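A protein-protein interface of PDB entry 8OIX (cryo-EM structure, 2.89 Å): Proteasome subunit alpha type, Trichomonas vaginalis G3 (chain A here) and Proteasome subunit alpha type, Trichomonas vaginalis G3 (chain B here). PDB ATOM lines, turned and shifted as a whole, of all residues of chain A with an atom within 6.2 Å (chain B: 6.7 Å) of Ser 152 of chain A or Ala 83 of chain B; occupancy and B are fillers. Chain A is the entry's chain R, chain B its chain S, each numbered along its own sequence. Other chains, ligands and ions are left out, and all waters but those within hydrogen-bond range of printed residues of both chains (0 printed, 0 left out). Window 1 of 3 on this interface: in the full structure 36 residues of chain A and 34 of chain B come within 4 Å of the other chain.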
ATOM      1  N   ILE A  20       9.678 -24.288  21.501  1.00  0.00           N
ATOM      2  CA  ILE A  20       9.912 -23.230  22.478  1.00  0.00           C
ATOM      3  C   ILE A  20       9.859 -23.784  23.895  1.00  0.00           C
ATOM      4  O   ILE A  20      10.626 -23.363  24.768  1.00  0.00           O
ATOM      5  CB  ILE A  20       8.908 -22.083  22.272  1.00  0.00           C
ATOM      6  CG1 ILE A  20       9.002 -21.572  20.839  1.00  0.00           C
ATOM      7  CG2 ILE A  20       9.171 -20.965  23.251  1.00  0.00           C
ATOM      8  CD1 ILE A  20      10.410 -21.315  20.404  1.00  0.00           C
ATOM      9  N   ALA A  23      13.224 -25.387  24.335  1.00  0.00           N
ATOM     10  CA  ALA A  23      14.248 -24.372  24.546  1.00  0.00           C
ATOM     11  C   ALA A  23      14.163 -23.790  25.953  1.00  0.00           C
ATOM     12  O   ALA A  23      15.191 -23.518  26.585  1.00  0.00           O
ATOM     13  CB  ALA A  23      14.122 -23.277  23.491  1.00  0.00           C
ATOM     14  N   HIS A  24      12.945 -23.591  26.462  1.00  0.00           N
ATOM     15  CA  HIS A  24      12.782 -23.169  27.848  1.00  0.00           C
ATOM     16  C   HIS A  24      13.315 -24.218  28.813  1.00  0.00           C
ATOM     17  O   HIS A  24      13.893 -23.877  29.849  1.00  0.00           O
ATOM     18  CB  HIS A  24      11.313 -22.864  28.142  1.00  0.00           C
ATOM     19  CG  HIS A  24      10.877 -21.505  27.694  1.00  0.00           C
ATOM     20  ND1 HIS A  24      10.163 -21.294  26.534  1.00  0.00           N
ATOM     21  CD2 HIS A  24      11.055 -20.285  28.253  1.00  0.00           C
ATOM     22  CE1 HIS A  24       9.919 -20.003  26.399  1.00  0.00           C
ATOM     23  NE2 HIS A  24      10.449 -19.369  27.428  1.00  0.00           N
ATOM     24  N   ALA A 113      16.101 -10.542  21.447  1.00  0.00           N
ATOM     25  CA  ALA A 113      14.815 -11.222  21.403  1.00  0.00           C
ATOM     26  C   ALA A 113      14.382 -11.492  19.971  1.00  0.00           C
ATOM     27  O   ALA A 113      13.775 -12.527  19.694  1.00  0.00           O
ATOM     28  CB  ALA A 113      13.759 -10.396  22.134  1.00  0.00           C
ATOM     29  N   GLN A 116      16.313 -14.522  18.686  1.00  0.00           N
ATOM     30  CA  GLN A 116      15.664 -15.737  19.168  1.00  0.00           C
ATOM     31  C   GLN A 116      14.363 -15.988  18.414  1.00  0.00           C
ATOM     32  O   GLN A 116      14.079 -17.117  17.999  1.00  0.00           O
ATOM     33  CB  GLN A 116      15.416 -15.631  20.671  1.00  0.00           C
ATOM     34  CG  GLN A 116      16.633 -15.979  21.508  1.00  0.00           C
ATOM     35  CD  GLN A 116      16.649 -15.279  22.849  1.00  0.00           C
ATOM     36  OE1 GLN A 116      16.362 -14.088  22.944  1.00  0.00           O
ATOM     37  NE2 GLN A 116      16.991 -16.018  23.896  1.00  0.00           N
ATOM     38  N   LEU A 117      13.587 -14.931  18.190  1.00  0.00           N
ATOM     39  CA  LEU A 117      12.327 -15.043  17.468  1.00  0.00           C
ATOM     40  C   LEU A 117      12.535 -15.503  16.032  1.00  0.00           C
ATOM     41  O   LEU A 117      11.772 -16.330  15.526  1.00  0.00           O
ATOM     42  CB  LEU A 117      11.611 -13.700  17.503  1.00  0.00           C
ATOM     43  CG  LEU A 117      10.425 -13.518  16.571  1.00  0.00           C
ATOM     44  CD1 LEU A 117       9.323 -14.515  16.871  1.00  0.00           C
ATOM     45  CD2 LEU A 117       9.951 -12.102  16.728  1.00  0.00           C
ATOM     46  N   THR A 120      12.980 -18.945  15.975  1.00  0.00           N
ATOM     47  CA  THR A 120      11.670 -19.584  16.090  1.00  0.00           C
ATOM     48  C   THR A 120      10.863 -19.498  14.799  1.00  0.00           C
ATOM     49  O   THR A 120       9.897 -20.249  14.637  1.00  0.00           O
ATOM     50  CB  THR A 120      10.847 -18.964  17.218  1.00  0.00           C
ATOM     51  OG1 THR A 120      10.355 -17.683  16.804  1.00  0.00           O
ATOM     52  CG2 THR A 120      11.678 -18.801  18.463  1.00  0.00           C
ATOM     53  N   GLN A 121      11.223 -18.592  13.892  1.00  0.00           N
ATOM     54  CA  GLN A 121      10.477 -18.371  12.661  1.00  0.00           C
ATOM     55  C   GLN A 121      11.190 -18.863  11.415  1.00  0.00           C
ATOM     56  O   GLN A 121      10.525 -19.182  10.430  1.00  0.00           O
ATOM     57  CB  GLN A 121      10.161 -16.881  12.485  1.00  0.00           C
ATOM     58  CG  GLN A 121       9.205 -16.309  13.516  1.00  0.00           C
ATOM     59  CD  GLN A 121       9.014 -14.813  13.361  1.00  0.00           C
ATOM     60  OE1 GLN A 121       9.836 -14.129  12.752  1.00  0.00           O
ATOM     61  NE2 GLN A 121       7.917 -14.297  13.904  1.00  0.00           N
ATOM     62  N   TYR A 128      16.963 -20.602  19.921  1.00  0.00           N
ATOM     63  CA  TYR A 128      18.028 -20.486  20.905  1.00  0.00           C
ATOM     64  C   TYR A 128      17.556 -21.045  22.237  1.00  0.00           C
ATOM     65  O   TYR A 128      16.563 -20.577  22.800  1.00  0.00           O
ATOM     66  CB  TYR A 128      18.455 -19.030  21.062  1.00  0.00           C
ATOM     67  CG  TYR A 128      19.271 -18.495  19.911  1.00  0.00           C
ATOM     68  CD1 TYR A 128      20.653 -18.616  19.899  1.00  0.00           C
ATOM     69  CD2 TYR A 128      18.662 -17.843  18.851  1.00  0.00           C
ATOM     70  CE1 TYR A 128      21.403 -18.120  18.854  1.00  0.00           C
ATOM     71  CE2 TYR A 128      19.404 -17.340  17.804  1.00  0.00           C
ATOM     72  CZ  TYR A 128      20.773 -17.482  17.809  1.00  0.00           C
ATOM     73  OH  TYR A 128      21.512 -16.982  16.763  1.00  0.00           O
ATOM     74  N   LEU A 150      13.462 -14.203  26.050  1.00  0.00           N
ATOM     75  CA  LEU A 150      13.194 -15.624  26.185  1.00  0.00           C
ATOM     76  C   LEU A 150      13.493 -16.346  24.883  1.00  0.00           C
ATOM     77  O   LEU A 150      13.663 -15.721  23.833  1.00  0.00           O
ATOM     78  CB  LEU A 150      11.735 -15.847  26.599  1.00  0.00           C
ATOM     79  CG  LEU A 150      11.273 -15.558  28.033  1.00  0.00           C
ATOM     80  CD1 LEU A 150      11.412 -14.093  28.425  1.00  0.00           C
ATOM     81  CD2 LEU A 150       9.838 -16.028  28.220  1.00  0.00           C
ATOM     82  N   PRO A 151      13.587 -17.678  24.916  1.00  0.00           N
ATOM     83  CA  PRO A 151      13.721 -18.427  23.656  1.00  0.00           C
ATOM     84  C   PRO A 151      12.588 -18.165  22.685  1.00  0.00           C
ATOM     85  O   PRO A 151      12.805 -18.200  21.468  1.00  0.00           O
ATOM     86  CB  PRO A 151      13.742 -19.887  24.120  1.00  0.00           C
ATOM     87  CG  PRO A 151      14.259 -19.828  25.499  1.00  0.00           C
ATOM     88  CD  PRO A 151      13.733 -18.558  26.089  1.00  0.00           C
ATOM     89  N   SER A 152      11.379 -17.910  23.190  1.00  0.00           N
ATOM     90  CA  SER A 152      10.258 -17.572  22.324  1.00  0.00           C
ATOM     91  C   SER A 152      10.520 -16.304  21.528  1.00  0.00           C
ATOM     92  O   SER A 152       9.857 -16.073  20.512  1.00  0.00           O
ATOM     93  CB  SER A 152       8.985 -17.409  23.153  1.00  0.00           C
ATOM     94  OG  SER A 152       9.152 -16.413  24.148  1.00  0.00           O
ATOM     95  N   GLY A 153      11.469 -15.486  21.964  1.00  0.00           N
ATOM     96  CA  GLY A 153      11.708 -14.199  21.361  1.00  0.00           C
ATOM     97  C   GLY A 153      11.006 -13.046  22.031  1.00  0.00           C
ATOM     98  O   GLY A 153      10.983 -11.949  21.467  1.00  0.00           O
ATOM     99  N   THR A 154      10.431 -13.257  23.209  1.00  0.00           N
ATOM    100  CA  THR A 154       9.773 -12.200  23.961  1.00  0.00           C
ATOM    101  C   THR A 154      10.753 -11.617  24.969  1.00  0.00           C
ATOM    102  O   THR A 154      11.445 -12.362  25.669  1.00  0.00           O
ATOM    103  CB  THR A 154       8.534 -12.733  24.682  1.00  0.00           C
ATOM    104  OG1 THR A 154       8.925 -13.750  25.611  1.00  0.00           O
ATOM    105  CG2 THR A 154       7.553 -13.323  23.684  1.00  0.00           C
ATOM    106  N   MET B  78      -1.928  -6.645  20.395  1.00  0.00           N
ATOM    107  CA  MET B  78      -1.666  -8.043  20.090  1.00  0.00           C
ATOM    108  C   MET B  78      -2.414  -8.971  21.039  1.00  0.00           C
ATOM    109  O   MET B  78      -2.810  -8.591  22.143  1.00  0.00           O
ATOM    110  CB  MET B  78      -0.170  -8.342  20.189  1.00  0.00           C
ATOM    111  CG  MET B  78       0.733  -7.215  19.752  1.00  0.00           C
ATOM    112  SD  MET B  78       2.454  -7.704  19.918  1.00  0.00           S
ATOM    113  CE  MET B  78       2.514  -8.112  21.660  1.00  0.00           C
ATOM    114  N   GLY B  80      -1.765 -13.301  21.877  1.00  0.00           N
ATOM    115  CA  GLY B  80      -1.121 -14.547  21.521  1.00  0.00           C
ATOM    116  C   GLY B  80       0.356 -14.549  21.842  1.00  0.00           C
ATOM    117  O   GLY B  80       0.748 -14.413  23.005  1.00  0.00           O
ATOM    118  N   LEU B  81       1.188 -14.704  20.817  1.00  0.00           N
ATOM    119  CA  LEU B  81       2.634 -14.700  20.987  1.00  0.00           C
ATOM    120  C   LEU B  81       3.139 -13.271  20.848  1.00  0.00           C
ATOM    121  O   LEU B  81       2.972 -12.648  19.795  1.00  0.00           O
ATOM    122  CB  LEU B  81       3.299 -15.611  19.960  1.00  0.00           C
ATOM    123  CG  LEU B  81       2.773 -17.043  19.924  1.00  0.00           C
ATOM    124  CD1 LEU B  81       3.445 -17.802  18.808  1.00  0.00           C
ATOM    125  CD2 LEU B  81       3.000 -17.731  21.257  1.00  0.00           C
ATOM    126  N   ALA B  82       3.751 -12.754  21.914  1.00  0.00           N
ATOM    127  CA  ALA B  82       4.201 -11.368  21.905  1.00  0.00           C
ATOM    128  C   ALA B  82       5.320 -11.141  20.898  1.00  0.00           C
ATOM    129  O   ALA B  82       5.446 -10.039  20.356  1.00  0.00           O
ATOM    130  CB  ALA B  82       4.651 -10.953  23.303  1.00  0.00           C
ATOM    131  N   ALA B  83       6.137 -12.162  20.633  1.00  0.00           N
ATOM    132  CA  ALA B  83       7.232 -12.002  19.682  1.00  0.00           C
ATOM    133  C   ALA B  83       6.729 -11.983  18.240  1.00  0.00           C
ATOM    134  O   ALA B  83       7.164 -11.150  17.435  1.00  0.00           O
ATOM    135  CB  ALA B  83       8.257 -13.113  19.887  1.00  0.00           C
ATOM    136  N   ASP B  84       5.812 -12.889  17.893  1.00  0.00           N
ATOM    137  CA  ASP B  84       5.218 -12.843  16.561  1.00  0.00           C
ATOM    138  C   ASP B  84       4.468 -11.536  16.353  1.00  0.00           C
ATOM    139  O   ASP B  84       4.523 -10.940  15.270  1.00  0.00           O
ATOM    140  CB  ASP B  84       4.286 -14.034  16.348  1.00  0.00           C
ATOM    141  CG  ASP B  84       4.988 -15.361  16.525  1.00  0.00           C
ATOM    142  OD1 ASP B  84       6.132 -15.370  17.024  1.00  0.00           O
ATOM    143  OD2 ASP B  84       4.399 -16.394  16.150  1.00  0.00           O
ATOM    144  N   GLY B  85       3.760 -11.078  17.383  1.00  0.00           N
ATOM    145  CA  GLY B  85       3.148  -9.768  17.316  1.00  0.00           C
ATOM    146  C   GLY B  85       4.158  -8.652  17.159  1.00  0.00           C
ATOM    147  O   GLY B  85       3.879  -7.653  16.499  1.00  0.00           O
ATOM    148  N   ARG B  86       5.336  -8.793  17.772  1.00  0.00           N
ATOM    149  CA  ARG B  86       6.388  -7.804  17.565  1.00  0.00           C
ATOM    150  C   ARG B  86       6.829  -7.774  16.111  1.00  0.00           C
ATOM    151  O   ARG B  86       7.049  -6.700  15.544  1.00  0.00           O
ATOM    152  CB  ARG B  86       7.587  -8.090  18.463  1.00  0.00           C
ATOM    153  CG  ARG B  86       8.666  -7.029  18.347  1.00  0.00           C
ATOM    154  CD  ARG B  86      10.026  -7.571  18.719  1.00  0.00           C
ATOM    155  NE  ARG B  86      10.031  -8.119  20.066  1.00  0.00           N
ATOM    156  CZ  ARG B  86      10.328  -9.376  20.355  1.00  0.00           C
ATOM    157  NH1 ARG B  86      10.721 -10.225  19.419  1.00  0.00           N
ATOM    158  NH2 ARG B  86      10.239  -9.792  21.613  1.00  0.00           N
ATOM    159  N   THR B  87       6.978  -8.946  15.496  1.00  0.00           N
ATOM    160  CA  THR B  87       7.308  -8.987  14.072  1.00  0.00           C
ATOM    161  C   THR B  87       6.218  -8.320  13.244  1.00  0.00           C
ATOM    162  O   THR B  87       6.506  -7.542  12.324  1.00  0.00           O
ATOM    163  CB  THR B  87       7.520 -10.429  13.610  1.00  0.00           C
ATOM    164  OG1 THR B  87       8.725 -10.941  14.182  1.00  0.00           O
ATOM    165  CG2 THR B  87       7.629 -10.495  12.099  1.00  0.00           C
ATOM    166  N   MET B  88       4.955  -8.608  13.566  1.00  0.00           N
ATOM    167  CA  MET B  88       3.846  -8.023  12.821  1.00  0.00           C
ATOM    168  C   MET B  88       3.822  -6.507  12.959  1.00  0.00           C
ATOM    169  O   MET B  88       3.644  -5.790  11.969  1.00  0.00           O
ATOM    170  CB  MET B  88       2.525  -8.630  13.291  1.00  0.00           C
ATOM    171  CG  MET B  88       2.413 -10.119  13.020  1.00  0.00           C
ATOM    172  SD  MET B  88       0.894 -10.873  13.625  1.00  0.00           S
ATOM    173  CE  MET B  88      -0.296 -10.238  12.450  1.00  0.00           C
ATOM    174  N   ARG B 137       6.340 -20.667  10.061  1.00  0.00           N
ATOM    175  CA  ARG B 137       5.091 -20.976  10.738  1.00  0.00           C
ATOM    176  C   ARG B 137       4.237 -19.722  10.751  1.00  0.00           C
ATOM    177  O   ARG B 137       4.778 -18.612  10.697  1.00  0.00           O
ATOM    178  CB  ARG B 137       5.341 -21.462  12.172  1.00  0.00           C
ATOM    179  CG  ARG B 137       6.232 -20.532  12.973  1.00  0.00           C
ATOM    180  CD  ARG B 137       6.144 -20.816  14.457  1.00  0.00           C
ATOM    181  NE  ARG B 137       6.914 -19.858  15.239  1.00  0.00           N
ATOM    182  CZ  ARG B 137       6.542 -18.605  15.468  1.00  0.00           C
ATOM    183  NH1 ARG B 137       5.407 -18.123  14.990  1.00  0.00           N
ATOM    184  NH2 ARG B 137       7.329 -17.818  16.196  1.00  0.00           N
ATOM    185  N   PHE B 139       2.043 -16.576  12.087  1.00  0.00           N
ATOM    186  CA  PHE B 139       2.126 -15.741  13.277  1.00  0.00           C
ATOM    187  C   PHE B 139       1.093 -16.194  14.295  1.00  0.00           C
ATOM    188  O   PHE B 139      -0.103 -16.232  14.002  1.00  0.00           O
ATOM    189  CB  PHE B 139       1.902 -14.278  12.906  1.00  0.00           C
ATOM    190  CG  PHE B 139       3.032 -13.670  12.135  1.00  0.00           C
ATOM    191  CD1 PHE B 139       4.343 -13.885  12.518  1.00  0.00           C
ATOM    192  CD2 PHE B 139       2.784 -12.889  11.021  1.00  0.00           C
ATOM    193  CE1 PHE B 139       5.384 -13.325  11.810  1.00  0.00           C
ATOM    194  CE2 PHE B 139       3.820 -12.328  10.309  1.00  0.00           C
ATOM    195  CZ  PHE B 139       5.122 -12.547  10.704  1.00  0.00           C
ATOM    196  N   THR B 141      -0.184 -14.668  16.540  1.00  0.00           N
ATOM    197  CA  THR B 141      -0.675 -13.429  17.119  1.00  0.00           C
ATOM    198  C   THR B 141      -1.828 -12.900  16.281  1.00  0.00           C
ATOM    199  O   THR B 141      -1.749 -12.884  15.049  1.00  0.00           O
ATOM    200  CB  THR B 141       0.433 -12.375  17.201  1.00  0.00           C
ATOM    201  OG1 THR B 141       1.523 -12.884  17.979  1.00  0.00           O
ATOM    202  CG2 THR B 141      -0.093 -11.113  17.856  1.00  0.00           C
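O of Thr 120 of chain A lies within hydrogen-bond range of NE of Arg 137 of chain B. NE2 of Gln 121 of chain A sits at hydrogen-bond distance from OG1 of Thr 87 of chain B (3.5 Å). The backbone carbonyl oxygen of Gly 153 of chain A sits at hydrogen-bond distance from the guanidinium group of Arg 86 of chain B (2.7 Å).
The side-chain hydroxyl of Ser 152 of chain A sits at hydrogen-bond distance from the side-chain hydroxyl of Thr 154 of chain A, at 3.0 Å. The backbone NH of Arg 86 of chain B sits at hydrogen-bond distance from the side-chain sulfur of Met 78 of chain B (3.8 Å). OD1 of Asp 84 of chain B lies within salt-bridge range of NH2 of Arg 137 of chain B (2.8 Å).
Ala 83 of chain B touches Leu 117 of chain A. Arg 86 of chain B touches Leu 117 of chain A (NH1 to CD2, 3.4 Å). Thr 87 of chain B touches Leu 117 of chain A. Leu 117 of chain A touches Arg 137 of chain B (CD1 to NH2, 3.9 Å). CG of Gln 121 of chain A touches NH2 of Arg 137 of chain B, 3.6 Å away. Phe 139 of chain B touches Gln 121 of chain A. Ala 83 of chain B touches Ser 152 of chain A (CB to O, 3.4 Å). CB of Ala 83 of chain B touches O of Gly 153 of chain A, 3.4 Å away. Thr 154 of chain A touches Ala 82 of chain B (CG2 to CB, 3.8 Å). Thr 154 of chain A touches Arg 86 of chain B.
Of the printed residues of chain B, Ala 113 of chain A touches Arg 86. Of the printed residues of chain B, Leu 117 of chain A touches Ala 83 (3.0 Å), Asp 84 (3.3 Å), Arg 86 (3.4 Å), Thr 87 (3.1 Å) and Arg 137 (3.9 Å). Of the printed residues of chain B, Thr 120 of chain A touches Arg 137 (3.1 Å). Printed residues of chain B within 4 Å of Gly 153 of chain A: Ala 83 (3.4 Å) and Arg 86 (2.3 Å). Of chain A, only Leu 117 (3.0 Å), Ser 152 (3.4 Å), Gly 153 (3.4 Å) and Thr 154 (3.6 Å) come within 4 Å of Ala 83 of chain B. The nearest residue of chain B that does not touch Ser 152 of chain A is Asp 84 of chain B (5.2 Å). The nearest printed residue of chain B that does not touch Leu 117 of chain A is Ala 82 of chain B (6.1 Å).
Of the 13 printed residues of chain B, 7 touch a printed residue of chain A. Printed residues of chain B that touch a printed residue of chain A: Ala 82, Ala 83, Asp 84, Arg 86, Thr 87, Arg 137 and Phe 139. Hydrophobic or aromatic side chains of chain B that line the printed part of chain A: Ala 82, Ala 83 and Phe 139. Of the 14 printed residues of chain A, 7 touch a printed residue of chain B. Hydrophobic or aromatic side chains of chain A that line the printed part of chain B: Ala 113 and Leu 117. Among the printed residues, 17 pairs touch across the chains. Among the printed residues, no Asp or Glu carboxylate lies within 4 Å of a Lys or Arg side-chain nitrogen of the other chain.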
